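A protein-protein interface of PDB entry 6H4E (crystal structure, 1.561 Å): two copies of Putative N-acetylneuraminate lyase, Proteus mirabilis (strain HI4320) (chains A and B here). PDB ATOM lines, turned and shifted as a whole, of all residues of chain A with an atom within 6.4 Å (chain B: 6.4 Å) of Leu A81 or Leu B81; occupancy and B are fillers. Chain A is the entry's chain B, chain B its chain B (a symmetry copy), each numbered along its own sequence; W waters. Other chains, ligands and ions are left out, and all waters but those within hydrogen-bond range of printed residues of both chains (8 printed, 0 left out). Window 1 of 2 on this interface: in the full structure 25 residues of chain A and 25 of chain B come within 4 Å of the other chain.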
ATOM      1  N   ILE A  50      21.717 -12.155  16.574  1.00  0.00           N
ATOM      2  CA  ILE A  50      21.362 -12.906  17.770  1.00  0.00           C
ATOM      3  C   ILE A  50      22.557 -13.595  18.401  1.00  0.00           C
ATOM      4  O   ILE A  50      22.422 -14.159  19.489  1.00  0.00           O
ATOM      5  CB  ILE A  50      20.232 -13.913  17.469  1.00  0.00           C
ATOM      6  CG1 ILE A  50      20.592 -14.772  16.249  1.00  0.00           C
ATOM      7  CG2 ILE A  50      18.902 -13.173  17.298  1.00  0.00           C
ATOM      8  CD1 ILE A  50      20.926 -16.201  16.562  1.00  0.00           C
ATOM      9  N   HIS A  51      23.733 -13.540  17.775  1.00  0.00           N
ATOM     10  CA  HIS A  51      24.936 -14.041  18.425  1.00  0.00           C
ATOM     11  C   HIS A  51      25.654 -12.986  19.249  1.00  0.00           C
ATOM     12  O   HIS A  51      26.596 -13.318  19.978  1.00  0.00           O
ATOM     13  CB  HIS A  51      25.891 -14.617  17.374  1.00  0.00           C
ATOM     14  CG  HIS A  51      25.423 -15.922  16.819  1.00  0.00           C
ATOM     15  ND1 HIS A  51      26.021 -16.540  15.740  1.00  0.00           N
ATOM     16  CD2 HIS A  51      24.435 -16.754  17.230  1.00  0.00           C
ATOM     17  CE1 HIS A  51      25.408 -17.687  15.500  1.00  0.00           C
ATOM     18  NE2 HIS A  51      24.438 -17.839  16.386  1.00  0.00           N
ATOM     19  N   CYS A  52      25.222 -11.738  19.169  1.00  0.00           N
ATOM     20  CA  CYS A  52      25.868 -10.632  19.854  1.00  0.00           C
ATOM     21  C   CYS A  52      25.069 -10.230  21.087  1.00  0.00           C
ATOM     22  O   CYS A  52      23.850 -10.393  21.130  1.00  0.00           O
ATOM     23  CB  CYS A  52      25.999  -9.442  18.904  1.00  0.00           C
ATOM     24  SG  CYS A  52      27.076  -9.798  17.489  1.00  0.00           S
ATOM     25  N   GLY A  79      15.580  -7.677  16.788  1.00  0.00           N
ATOM     26  CA  GLY A  79      14.882  -8.820  17.352  1.00  0.00           C
ATOM     27  C   GLY A  79      15.767  -9.669  18.247  1.00  0.00           C
ATOM     28  O   GLY A  79      16.953  -9.868  17.995  1.00  0.00           O
ATOM     29  N   ALA A  80      15.148 -10.206  19.298  1.00  0.00           N
ATOM     30  CA  ALA A  80      15.805 -11.074  20.267  1.00  0.00           C
ATOM     31  C   ALA A  80      14.718 -11.896  20.939  1.00  0.00           C
ATOM     32  O   ALA A  80      13.541 -11.537  20.890  1.00  0.00           O
ATOM     33  CB  ALA A  80      16.585 -10.266  21.306  1.00  0.00           C
ATOM     34  N   LEU A  81      15.117 -13.005  21.563  1.00  0.00           N
ATOM     35  CA  LEU A  81      14.103 -13.809  22.244  1.00  0.00           C
ATOM     36  C   LEU A  81      13.523 -13.077  23.445  1.00  0.00           C
ATOM     37  O   LEU A  81      12.357 -13.304  23.792  1.00  0.00           O
ATOM     38  CB  LEU A  81      14.673 -15.155  22.682  1.00  0.00           C
ATOM     39  CG  LEU A  81      14.990 -16.167  21.570  1.00  0.00           C
ATOM     40  CD1 LEU A  81      15.467 -17.479  22.173  1.00  0.00           C
ATOM     41  CD2 LEU A  81      13.793 -16.394  20.652  1.00  0.00           C
ATOM     42  N   SER A  82      14.295 -12.186  24.078  1.00  0.00           N
ATOM     43  CA  SER A  82      13.811 -11.434  25.233  1.00  0.00           C
ATOM     44  C   SER A  82      13.232 -10.101  24.780  1.00  0.00           C
ATOM     45  O   SER A  82      13.933  -9.302  24.148  1.00  0.00           O
ATOM     46  CB  SER A  82      14.923 -11.184  26.253  1.00  0.00           C
ATOM     47  OG  SER A  82      14.528 -10.165  27.169  1.00  0.00           O
ATOM     48  N   ILE A  83      11.964  -9.854  25.131  1.00  0.00           N
ATOM     49  CA  ILE A  83      11.340  -8.568  24.828  1.00  0.00           C
ATOM     50  C   ILE A  83      12.086  -7.438  25.532  1.00  0.00           C
ATOM     51  O   ILE A  83      12.126  -6.307  25.032  1.00  0.00           O
ATOM     52  CB  ILE A  83       9.836  -8.608  25.202  1.00  0.00           C
ATOM     53  CG1 ILE A  83       9.095  -7.347  24.737  1.00  0.00           C
ATOM     54  CG2 ILE A  83       9.643  -8.861  26.685  1.00  0.00           C
ATOM     55  CD1 ILE A  83       9.020  -7.225  23.227  1.00  0.00           C
ATOM     56  N   ALA A  84      12.706  -7.718  26.684  1.00  0.00           N
ATOM     57  CA  ALA A  84      13.497  -6.691  27.351  1.00  0.00           C
ATOM     58  C   ALA A  84      14.675  -6.270  26.483  1.00  0.00           C
ATOM     59  O   ALA A  84      14.920  -5.079  26.287  1.00  0.00           O
ATOM     60  CB  ALA A  84      13.976  -7.193  28.718  1.00  0.00           C
ATOM     61  N   ASP A  85      15.409  -7.246  25.942  1.00  0.00           N
ATOM     62  CA  ASP A  85      16.499  -6.941  25.019  1.00  0.00           C
ATOM     63  C   ASP A  85      15.995  -6.225  23.771  1.00  0.00           C
ATOM     64  O   ASP A  85      16.614  -5.257  23.309  1.00  0.00           O
ATOM     65  CB  ASP A  85      17.217  -8.228  24.602  1.00  0.00           C
ATOM     66  CG  ASP A  85      18.037  -8.854  25.716  1.00  0.00           C
ATOM     67  OD1 ASP A  85      18.230  -8.221  26.783  1.00  0.00           O
ATOM     68  OD2 ASP A  85      18.517  -9.987  25.484  1.00  0.00           O
ATOM     69  N   THR A  86      14.891  -6.710  23.191  1.00  0.00           N
ATOM     70  CA  THR A  86      14.379  -6.124  21.951  1.00  0.00           C
ATOM     71  C   THR A  86      14.020  -4.658  22.148  1.00  0.00           C
ATOM     72  O   THR A  86      14.357  -3.802  21.318  1.00  0.00           O
ATOM     73  CB  THR A  86      13.160  -6.909  21.468  1.00  0.00           C
ATOM     74  OG1 THR A  86      13.552  -8.247  21.145  1.00  0.00           O
ATOM     75  CG2 THR A  86      12.527  -6.253  20.229  1.00  0.00           C
ATOM     76  N   GLY A 105      10.624 -13.225  13.518  1.00  0.00           N
ATOM     77  CA  GLY A 105       9.685 -13.960  14.339  1.00  0.00           C
ATOM     78  C   GLY A 105      10.390 -14.744  15.427  1.00  0.00           C
ATOM     79  O   GLY A 105      11.366 -15.458  15.171  1.00  0.00           O
ATOM     80  N   PRO A 106       9.915 -14.617  16.668  1.00  0.00           N
ATOM     81  CA  PRO A 106      10.484 -15.405  17.770  1.00  0.00           C
ATOM     82  C   PRO A 106      10.370 -16.892  17.481  1.00  0.00           C
ATOM     83  O   PRO A 106       9.309 -17.382  17.082  1.00  0.00           O
ATOM     84  CB  PRO A 106       9.633 -14.988  18.978  1.00  0.00           C
ATOM     85  CG  PRO A 106       9.097 -13.631  18.615  1.00  0.00           C
ATOM     86  CD  PRO A 106       8.857 -13.699  17.124  1.00  0.00           C
ATOM     87  N   CYS A 107      11.473 -17.614  17.686  1.00  0.00           N
ATOM     88  CA  CYS A 107      11.597 -18.969  17.176  1.00  0.00           C
ATOM     89  C   CYS A 107      11.565 -20.048  18.249  1.00  0.00           C
ATOM     90  O   CYS A 107      11.688 -21.228  17.907  1.00  0.00           O
ATOM     91  CB  CYS A 107      12.885 -19.099  16.355  1.00  0.00           C
ATOM     92  SG  CYS A 107      14.383 -18.915  17.332  1.00  0.00           S
ATOM     93  N   PHE A 108      11.398 -19.694  19.523  1.00  0.00           N
ATOM     94  CA  PHE A 108      11.333 -20.732  20.545  1.00  0.00           C
ATOM     95  C   PHE A 108       9.892 -20.959  20.980  1.00  0.00           C
ATOM     96  O   PHE A 108       9.302 -21.989  20.642  1.00  0.00           O
ATOM     97  CB  PHE A 108      12.218 -20.397  21.741  1.00  0.00           C
ATOM     98  CG  PHE A 108      12.348 -21.539  22.704  1.00  0.00           C
ATOM     99  CD1 PHE A 108      13.090 -22.662  22.371  1.00  0.00           C
ATOM    100  CD2 PHE A 108      11.688 -21.507  23.922  1.00  0.00           C
ATOM    101  CE1 PHE A 108      13.191 -23.724  23.248  1.00  0.00           C
ATOM    102  CE2 PHE A 108      11.794 -22.562  24.808  1.00  0.00           C
ATOM    103  CZ  PHE A 108      12.545 -23.671  24.469  1.00  0.00           C
ATOM    104  N   PHE A 109       9.329 -20.022  21.741  1.00  0.00           N
ATOM    105  CA  PHE A 109       7.876 -19.938  21.870  1.00  0.00           C
ATOM    106  C   PHE A 109       7.357 -19.336  20.571  1.00  0.00           C
ATOM    107  O   PHE A 109       7.410 -18.121  20.373  1.00  0.00           O
ATOM    108  CB  PHE A 109       7.476 -19.074  23.063  1.00  0.00           C
ATOM    109  CG  PHE A 109       7.878 -19.628  24.409  1.00  0.00           C
ATOM    110  CD1 PHE A 109       7.254 -20.743  24.940  1.00  0.00           C
ATOM    111  CD2 PHE A 109       8.846 -18.989  25.165  1.00  0.00           C
ATOM    112  CE1 PHE A 109       7.610 -21.224  26.187  1.00  0.00           C
ATOM    113  CE2 PHE A 109       9.203 -19.464  26.418  1.00  0.00           C
ATOM    114  CZ  PHE A 109       8.590 -20.573  26.928  1.00  0.00           C
ATOM    115  N   TYR A 120       3.576  -8.620  19.467  1.00  0.00           N
ATOM    116  CA  TYR A 120       5.021  -8.590  19.647  1.00  0.00           C
ATOM    117  C   TYR A 120       5.657  -7.512  18.771  1.00  0.00           C
ATOM    118  O   TYR A 120       6.448  -6.691  19.253  1.00  0.00           O
ATOM    119  CB  TYR A 120       5.608  -9.976  19.340  1.00  0.00           C
ATOM    120  CG  TYR A 120       7.118 -10.007  19.332  1.00  0.00           C
ATOM    121  CD1 TYR A 120       7.843  -9.998  20.520  1.00  0.00           C
ATOM    122  CD2 TYR A 120       7.826 -10.030  18.135  1.00  0.00           C
ATOM    123  CE1 TYR A 120       9.223 -10.013  20.519  1.00  0.00           C
ATOM    124  CE2 TYR A 120       9.202 -10.040  18.124  1.00  0.00           C
ATOM    125  CZ  TYR A 120       9.904 -10.037  19.311  1.00  0.00           C
ATOM    126  OH  TYR A 120      11.284 -10.046  19.301  1.00  0.00           O
ATOM    127  N   ARG A 272      30.272 -19.352  17.540  1.00  0.00           N
ATOM    128  CA  ARG A 272      29.577 -20.532  18.028  1.00  0.00           C
ATOM    129  C   ARG A 272      28.149 -20.136  18.419  1.00  0.00           C
ATOM    130  O   ARG A 272      27.941 -19.048  18.959  1.00  0.00           O
ATOM    131  CB  ARG A 272      30.327 -21.134  19.228  1.00  0.00           C
ATOM    132  CG  ARG A 272      31.709 -21.690  18.878  1.00  0.00           C
ATOM    133  CD  ARG A 272      31.599 -22.993  18.115  1.00  0.00           C
ATOM    134  NE  ARG A 272      32.908 -23.505  17.707  1.00  0.00           N
ATOM    135  CZ  ARG A 272      33.083 -24.643  17.041  1.00  0.00           C
ATOM    136  NH1 ARG A 272      32.035 -25.380  16.711  1.00  0.00           N
ATOM    137  NH2 ARG A 272      34.309 -25.043  16.710  1.00  0.00           N
ATOM    138  N   PRO A 273      27.164 -21.020  18.186  1.00  0.00           N
ATOM    139  CA  PRO A 273      27.252 -22.433  17.787  1.00  0.00           C
ATOM    140  C   PRO A 273      27.538 -22.728  16.323  1.00  0.00           C
ATOM    141  O   PRO A 273      27.663 -23.900  16.006  1.00  0.00           O
ATOM    142  CB  PRO A 273      25.864 -22.974  18.147  1.00  0.00           C
ATOM    143  CG  PRO A 273      24.970 -21.804  17.969  1.00  0.00           C
ATOM    144  CD  PRO A 273      25.771 -20.625  18.468  1.00  0.00           C
ATOM    145  N   ILE B  50      14.753 -17.253  28.701  1.00  0.00           N
ATOM    146  CA  ILE B  50      15.080 -16.546  27.471  1.00  0.00           C
ATOM    147  C   ILE B  50      14.218 -15.317  27.257  1.00  0.00           C
ATOM    148  O   ILE B  50      14.474 -14.556  26.321  1.00  0.00           O
ATOM    149  CB  ILE B  50      15.006 -17.497  26.257  1.00  0.00           C
ATOM    150  CG1 ILE B  50      13.662 -18.238  26.239  1.00  0.00           C
ATOM    151  CG2 ILE B  50      16.206 -18.450  26.263  1.00  0.00           C
ATOM    152  CD1 ILE B  50      12.718 -17.802  25.158  1.00  0.00           C
ATOM    153  N   HIS B  51      13.225 -15.074  28.113  1.00  0.00           N
ATOM    154  CA  HIS B  51      12.483 -13.823  28.043  1.00  0.00           C
ATOM    155  C   HIS B  51      13.093 -12.719  28.890  1.00  0.00           C
ATOM    156  O   HIS B  51      12.656 -11.567  28.796  1.00  0.00           O
ATOM    157  CB  HIS B  51      11.029 -14.059  28.467  1.00  0.00           C
ATOM    158  CG  HIS B  51      10.239 -14.799  27.440  1.00  0.00           C
ATOM    159  ND1 HIS B  51       8.966 -15.279  27.669  1.00  0.00           N
ATOM    160  CD2 HIS B  51      10.529 -15.102  26.151  1.00  0.00           C
ATOM    161  CE1 HIS B  51       8.515 -15.862  26.571  1.00  0.00           C
ATOM    162  NE2 HIS B  51       9.445 -15.774  25.635  1.00  0.00           N
ATOM    163  N   CYS B  52      14.099 -13.036  29.690  1.00  0.00           N
ATOM    164  CA  CYS B  52      14.718 -12.085  30.597  1.00  0.00           C
ATOM    165  C   CYS B  52      16.055 -11.612  30.041  1.00  0.00           C
ATOM    166  O   CYS B  52      16.726 -12.339  29.309  1.00  0.00           O
ATOM    167  CB  CYS B  52      14.919 -12.732  31.966  1.00  0.00           C
ATOM    168  SG  CYS B  52      13.352 -13.174  32.764  1.00  0.00           S
ATOM    169  N   GLY B  79      21.431 -20.851  29.167  1.00  0.00           N
ATOM    170  CA  GLY B  79      21.422 -20.857  27.714  1.00  0.00           C
ATOM    171  C   GLY B  79      20.778 -19.616  27.122  1.00  0.00           C
ATOM    172  O   GLY B  79      19.802 -19.078  27.637  1.00  0.00           O
ATOM    173  N   ALA B  80      21.332 -19.185  25.989  1.00  0.00           N
ATOM    174  CA  ALA B  80      20.853 -18.028  25.244  1.00  0.00           C
ATOM    175  C   ALA B  80      21.336 -18.189  23.812  1.00  0.00           C
ATOM    176  O   ALA B  80      22.263 -18.955  23.546  1.00  0.00           O
ATOM    177  CB  ALA B  80      21.374 -16.721  25.842  1.00  0.00           C
ATOM    178  N   LEU B  81      20.700 -17.464  22.890  1.00  0.00           N
ATOM    179  CA  LEU B  81      21.154 -17.572  21.504  1.00  0.00           C
ATOM    180  C   LEU B  81      22.544 -16.985  21.324  1.00  0.00           C
ATOM    181  O   LEU B  81      23.291 -17.441  20.448  1.00  0.00           O
ATOM    182  CB  LEU B  81      20.175 -16.891  20.552  1.00  0.00           C
ATOM    183  CG  LEU B  81      18.815 -17.576  20.351  1.00  0.00           C
ATOM    184  CD1 LEU B  81      17.993 -16.823  19.317  1.00  0.00           C
ATOM    185  CD2 LEU B  81      18.970 -19.042  19.960  1.00  0.00           C
ATOM    186  N   SER B  82      22.927 -15.998  22.143  1.00  0.00           N
ATOM    187  CA  SER B  82      24.251 -15.387  22.043  1.00  0.00           C
ATOM    188  C   SER B  82      25.219 -16.085  22.987  1.00  0.00           C
ATOM    189  O   SER B  82      24.979 -16.134  24.199  1.00  0.00           O
ATOM    190  CB  SER B  82      24.210 -13.893  22.372  1.00  0.00           C
ATOM    191  OG  SER B  82      25.529 -13.410  22.618  1.00  0.00           O
ATOM    192  N   ILE B  83      26.324 -16.596  22.431  1.00  0.00           N
ATOM    193  CA  ILE B  83      27.364 -17.207  23.257  1.00  0.00           C
ATOM    194  C   ILE B  83      27.946 -16.179  24.222  1.00  0.00           C
ATOM    195  O   ILE B  83      28.384 -16.532  25.324  1.00  0.00           O
ATOM    196  CB  ILE B  83      28.448 -17.851  22.354  1.00  0.00           C
ATOM    197  CG1 ILE B  83      29.466 -18.661  23.167  1.00  0.00           C
ATOM    198  CG2 ILE B  83      29.123 -16.813  21.478  1.00  0.00           C
ATOM    199  CD1 ILE B  83      28.861 -19.889  23.823  1.00  0.00           C
ATOM    200  N   ALA B  84      27.943 -14.894  23.847  1.00  0.00           N
ATOM    201  CA  ALA B  84      28.415 -13.868  24.769  1.00  0.00           C
ATOM    202  C   ALA B  84      27.531 -13.810  26.008  1.00  0.00           C
ATOM    203  O   ALA B  84      28.028 -13.796  27.135  1.00  0.00           O
ATOM    204  CB  ALA B  84      28.465 -12.506  24.067  1.00  0.00           C
ATOM    205  N   ASP B  85      26.211 -13.788  25.810  1.00  0.00           N
ATOM    206  CA  ASP B  85      25.284 -13.828  26.939  1.00  0.00           C
ATOM    207  C   ASP B  85      25.440 -15.110  27.748  1.00  0.00           C
ATOM    208  O   ASP B  85      25.438 -15.075  28.986  1.00  0.00           O
ATOM    209  CB  ASP B  85      23.839 -13.723  26.441  1.00  0.00           C
ATOM    210  CG  ASP B  85      23.479 -12.348  25.906  1.00  0.00           C
ATOM    211  OD1 ASP B  85      24.268 -11.386  26.074  1.00  0.00           O
ATOM    212  OD2 ASP B  85      22.367 -12.245  25.342  1.00  0.00           O
ATOM    213  N   THR B  86      25.541 -16.257  27.066  1.00  0.00           N
ATOM    214  CA  THR B  86      25.624 -17.539  27.768  1.00  0.00           C
ATOM    215  C   THR B  86      26.853 -17.591  28.665  1.00  0.00           C
ATOM    216  O   THR B  86      26.777 -18.021  29.824  1.00  0.00           O
ATOM    217  CB  THR B  86      25.656 -18.685  26.756  1.00  0.00           C
ATOM    218  OG1 THR B  86      24.426 -18.710  26.025  1.00  0.00           O
ATOM    219  CG2 THR B  86      25.858 -20.041  27.455  1.00  0.00           C
ATOM    220  N   GLY B 105      19.463 -26.560  23.729  1.00  0.00           N
ATOM    221  CA  GLY B 105      19.981 -26.511  22.377  1.00  0.00           C
ATOM    222  C   GLY B 105      19.582 -25.229  21.674  1.00  0.00           C
ATOM    223  O   GLY B 105      18.412 -24.832  21.687  1.00  0.00           O
ATOM    224  N   PRO B 106      20.552 -24.553  21.056  1.00  0.00           N
ATOM    225  CA  PRO B 106      20.240 -23.345  20.278  1.00  0.00           C
ATOM    226  C   PRO B 106      19.246 -23.660  19.173  1.00  0.00           C
ATOM    227  O   PRO B 106      19.404 -24.638  18.436  1.00  0.00           O
ATOM    228  CB  PRO B 106      21.607 -22.924  19.718  1.00  0.00           C
ATOM    229  CG  PRO B 106      22.607 -23.525  20.665  1.00  0.00           C
ATOM    230  CD  PRO B 106      21.996 -24.843  21.085  1.00  0.00           C
ATOM    231  N   CYS B 107      18.215 -22.822  19.058  1.00  0.00           N
ATOM    232  CA  CYS B 107      17.050 -23.160  18.259  1.00  0.00           C
ATOM    233  C   CYS B 107      16.915 -22.353  16.976  1.00  0.00           C
ATOM    234  O   CYS B 107      15.940 -22.557  16.245  1.00  0.00           O
ATOM    235  CB  CYS B 107      15.778 -23.002  19.101  1.00  0.00           C
ATOM    236  SG  CYS B 107      15.439 -21.303  19.580  1.00  0.00           S
ATOM    237  N   PHE B 108      17.852 -21.455  16.669  1.00  0.00           N
ATOM    238  CA  PHE B 108      17.737 -20.708  15.422  1.00  0.00           C
ATOM    239  C   PHE B 108      18.695 -21.266  14.379  1.00  0.00           C
ATOM    240  O   PHE B 108      18.256 -21.911  13.423  1.00  0.00           O
ATOM    241  CB  PHE B 108      17.975 -19.218  15.638  1.00  0.00           C
ATOM    242  CG  PHE B 108      17.648 -18.396  14.428  1.00  0.00           C
ATOM    243  CD1 PHE B 108      16.331 -18.209  14.037  1.00  0.00           C
ATOM    244  CD2 PHE B 108      18.662 -17.853  13.654  1.00  0.00           C
ATOM    245  CE1 PHE B 108      16.029 -17.471  12.908  1.00  0.00           C
ATOM    246  CE2 PHE B 108      18.366 -17.105  12.530  1.00  0.00           C
ATOM    247  CZ  PHE B 108      17.050 -16.917  12.157  1.00  0.00           C
ATOM    248  N   PHE B 109      19.992 -21.010  14.541  1.00  0.00           N
ATOM    249  CA  PHE B 109      21.004 -21.812  13.857  1.00  0.00           C
ATOM    250  C   PHE B 109      21.073 -23.145  14.591  1.00  0.00           C
ATOM    251  O   PHE B 109      21.702 -23.253  15.645  1.00  0.00           O
ATOM    252  CB  PHE B 109      22.362 -21.117  13.870  1.00  0.00           C
ATOM    253  CG  PHE B 109      22.417 -19.820  13.098  1.00  0.00           C
ATOM    254  CD1 PHE B 109      22.364 -19.806  11.716  1.00  0.00           C
ATOM    255  CD2 PHE B 109      22.582 -18.619  13.766  1.00  0.00           C
ATOM    256  CE1 PHE B 109      22.445 -18.614  11.019  1.00  0.00           C
ATOM    257  CE2 PHE B 109      22.668 -17.421  13.072  1.00  0.00           C
ATOM    258  CZ  PHE B 109      22.602 -17.417  11.708  1.00  0.00           C
ATOM    259  N   TYR B 120      29.544 -26.235  21.594  1.00  0.00           N
ATOM    260  CA  TYR B 120      28.757 -25.195  22.242  1.00  0.00           C
ATOM    261  C   TYR B 120      28.614 -25.472  23.737  1.00  0.00           C
ATOM    262  O   TYR B 120      28.868 -24.593  24.570  1.00  0.00           O
ATOM    263  CB  TYR B 120      27.384 -25.086  21.561  1.00  0.00           C
ATOM    264  CG  TYR B 120      26.429 -24.153  22.266  1.00  0.00           C
ATOM    265  CD1 TYR B 120      26.559 -22.772  22.153  1.00  0.00           C
ATOM    266  CD2 TYR B 120      25.402 -24.650  23.061  1.00  0.00           C
ATOM    267  CE1 TYR B 120      25.697 -21.914  22.806  1.00  0.00           C
ATOM    268  CE2 TYR B 120      24.540 -23.802  23.721  1.00  0.00           C
ATOM    269  CZ  TYR B 120      24.680 -22.437  23.592  1.00  0.00           C
ATOM    270  OH  TYR B 120      23.819 -21.586  24.254  1.00  0.00           O
ATOM    271  N   ARG B 272       5.458 -11.258  26.805  1.00  0.00           N
ATOM    272  CA  ARG B 272       5.389 -11.323  25.354  1.00  0.00           C
ATOM    273  C   ARG B 272       6.704 -11.901  24.822  1.00  0.00           C
ATOM    274  O   ARG B 272       7.769 -11.595  25.361  1.00  0.00           O
ATOM    275  CB  ARG B 272       5.128  -9.924  24.770  1.00  0.00           C
ATOM    276  CG  ARG B 272       3.761  -9.344  25.138  1.00  0.00           C
ATOM    277  CD  ARG B 272       2.651 -10.026  24.367  1.00  0.00           C
ATOM    278  NE  ARG B 272       1.327  -9.536  24.757  1.00  0.00           N
ATOM    279  CZ  ARG B 272       0.191  -9.962  24.213  1.00  0.00           C
ATOM    280  NH1 ARG B 272       0.220 -10.881  23.261  1.00  0.00           N
ATOM    281  NH2 ARG B 272      -0.975  -9.463  24.621  1.00  0.00           N
ATOM    282  N   PRO B 273       6.650 -12.707  23.748  1.00  0.00           N
ATOM    283  CA  PRO B 273       5.524 -12.981  22.841  1.00  0.00           C
ATOM    284  C   PRO B 273       4.460 -13.952  23.326  1.00  0.00           C
ATOM    285  O   PRO B 273       3.501 -14.136  22.594  1.00  0.00           O
ATOM    286  CB  PRO B 273       6.218 -13.569  21.608  1.00  0.00           C
ATOM    287  CG  PRO B 273       7.412 -14.250  22.164  1.00  0.00           C
ATOM    288  CD  PRO B 273       7.891 -13.348  23.276  1.00  0.00           C
HETATM  289  O   HOH W   1      10.545 -15.455  22.915  1.00  0.00           O
HETATM  290  O   HOH W   2      20.923 -10.216  23.965  1.00  0.00           O
HETATM  291  O   HOH W   3      22.648 -19.281  18.239  1.00  0.00           O
HETATM  292  O   HOH W   4      26.136 -17.210  19.767  1.00  0.00           O
HETATM  293  O   HOH W   5       4.918 -17.001  21.300  1.00  0.00           O
HETATM  294  O   HOH W   6      10.416 -12.064  25.611  1.00  0.00           O
HETATM  295  O   HOH W   7      20.007 -11.939  26.921  1.00  0.00           O
HETATM  296  O   HOH W   8      24.382 -24.065  14.957  1.00  0.00           O
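Water W4 lies within hydrogen-bond range of the backbone carbonyl oxygen (O) of Arg A272 (2.7 Å), the backbone NH (N) of Ile B83 (2.7 Å) and the backbone carbonyl oxygen (O) of Leu B81 (2.9 Å). Water W6 lies within hydrogen-bond range of O of Arg B272 (2.7 Å), N of Ile A83 (2.7 Å) and O of Leu A81 (2.9 Å). Water W7 bridges OD2 of Asp A85 (2.8 Å) and OD2 of Asp B85 (2.9 Å). Water W8 bridges O of Phe B109 (2.9 Å) and O of Pro A273 (3.4 Å). Water W1 bridges the backbone carbonyl oxygen (O) of Leu A81 (2.9 Å) and a ring nitrogen (NE2) of His B51 (3.0 Å). Water W3 bridges the backbone carbonyl oxygen (O) of Leu B81 (2.9 Å) and a ring nitrogen (NE2) of His A51 (3.0 Å).
Of the 19 printed residues of chain A, 12 touch a printed residue of chain B. Printed residues of chain A that touch a printed residue of chain B: Ile A50, His A51, Cys A52, Leu A81, Ser A82, Ile A83, Pro A106, Cys A107, Phe A108, Phe A109, Arg A272 and Pro A273. Hydrophobic or aromatic side chains of chain A that line the printed part of chain B: His A51, Leu A81, Ile A83, Pro A106, Phe A108, Phe A109 and Pro A273. Of the 19 printed residues of chain B, 12 touch a printed residue of chain A. Hydrophobic or aromatic side chains of chain B within 4 Å of the printed part of chain A: His B51, Leu B81, Ile B83, Pro B106, Phe B108, Phe B109 and Pro B273. Among the printed residues, 20 pairs touch across the chains.
Of the printed residues of chain B, Ile A50 touches Leu B81 and Ser B82. Of the printed residues of chain B, Cys A52 touches Ser B82. Of chain B, only Ile B50, His B51 and Leu B81 come within 4 Å of Leu A81. Asp A85 touches none of the printed residues of chain B. Of the printed residues of chain B, Arg A272 touches Ile B83 (3.6 Å). Leu B81 touches three residues of chain A. Of the printed residues of chain A, Pro B106 touches Pro A273. Tyr B120 touches none of the printed residues of chain A. Of the printed residues of chain A, Pro B273 touches Pro A106 (3.95 Å). The nearest printed residue of chain B that does not touch Phe A109 is Ile B50 (4.05 Å).
Ile A50 touches Ser B82, and with the chains exchanged Ser A82 touches Ile B50. His A51 touches Phe B109, and with the chains exchanged Phe A109 touches His B51. Ile A83 touches Arg B272, and with the chains exchanged Arg A272 touches Ile B83. Cys A107 touches Phe B108, and with the chains exchanged Phe A108 touches Cys B107. Of the 20 pairs that touch across the chains among the printed residues, 20 have their exchanged pair printed and touching as well.
OG of Ser A82 is in hydrogen-bond range of N of Asp A85 (3.3 Å). N of Ala B84 sits at hydrogen-bond distance from OG of Ser B82. O of Ser A82 sits at hydrogen-bond distance from OG1 of Thr A86 (3.2 Å). O of Ser B82 is in hydrogen-bond range of OG1 of Thr B86, 3.2 Å away. The side-chain hydroxyl (OG) of Ser B82 is in hydrogen-bond range of the backbone NH (N) of Asp B85. OG of Ser A82 lies within hydrogen-bond range of N of Ala A84 (3.1 Å).
Ile A50 touches Leu B81. Leu B81 touches His A51. O of Ile B50 touches C of Leu A81, 3.4 Å away. Leu A81 touches His B51. CG of Leu A81 touches CD1 of Leu B81, at 3.8 Å. OG of Ser A82 touches C of Cys B52 (3.6 Å). SG of Cys A107 touches CD1 of Phe B108, 3.9 Å away. Cys B107 touches Phe A108. CD2 of Phe A109 touches NE2 of His B51, 3.3 Å away. Pro B106 touches Pro A273 (CB to CG, 3.95 Å).
The side-chain hydroxyl of Ser B82 is in hydrogen-bond range of the backbone carbonyl oxygen of His A51. The backbone carbonyl oxygen (O) of His B51 sits at hydrogen-bond distance from the side-chain hydroxyl (OG) of Ser A82. SG of Cys A107 sits at hydrogen-bond distance from SG of Cys B107 (3.4 Å). N of Ser B82 lies within hydrogen-bond range of O of Ile A50 (3.3 Å). The backbone NH (N) of Ser A82 sits at hydrogen-bond distance from the backbone carbonyl oxygen (O) of Ile B50, at 3.3 Å.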
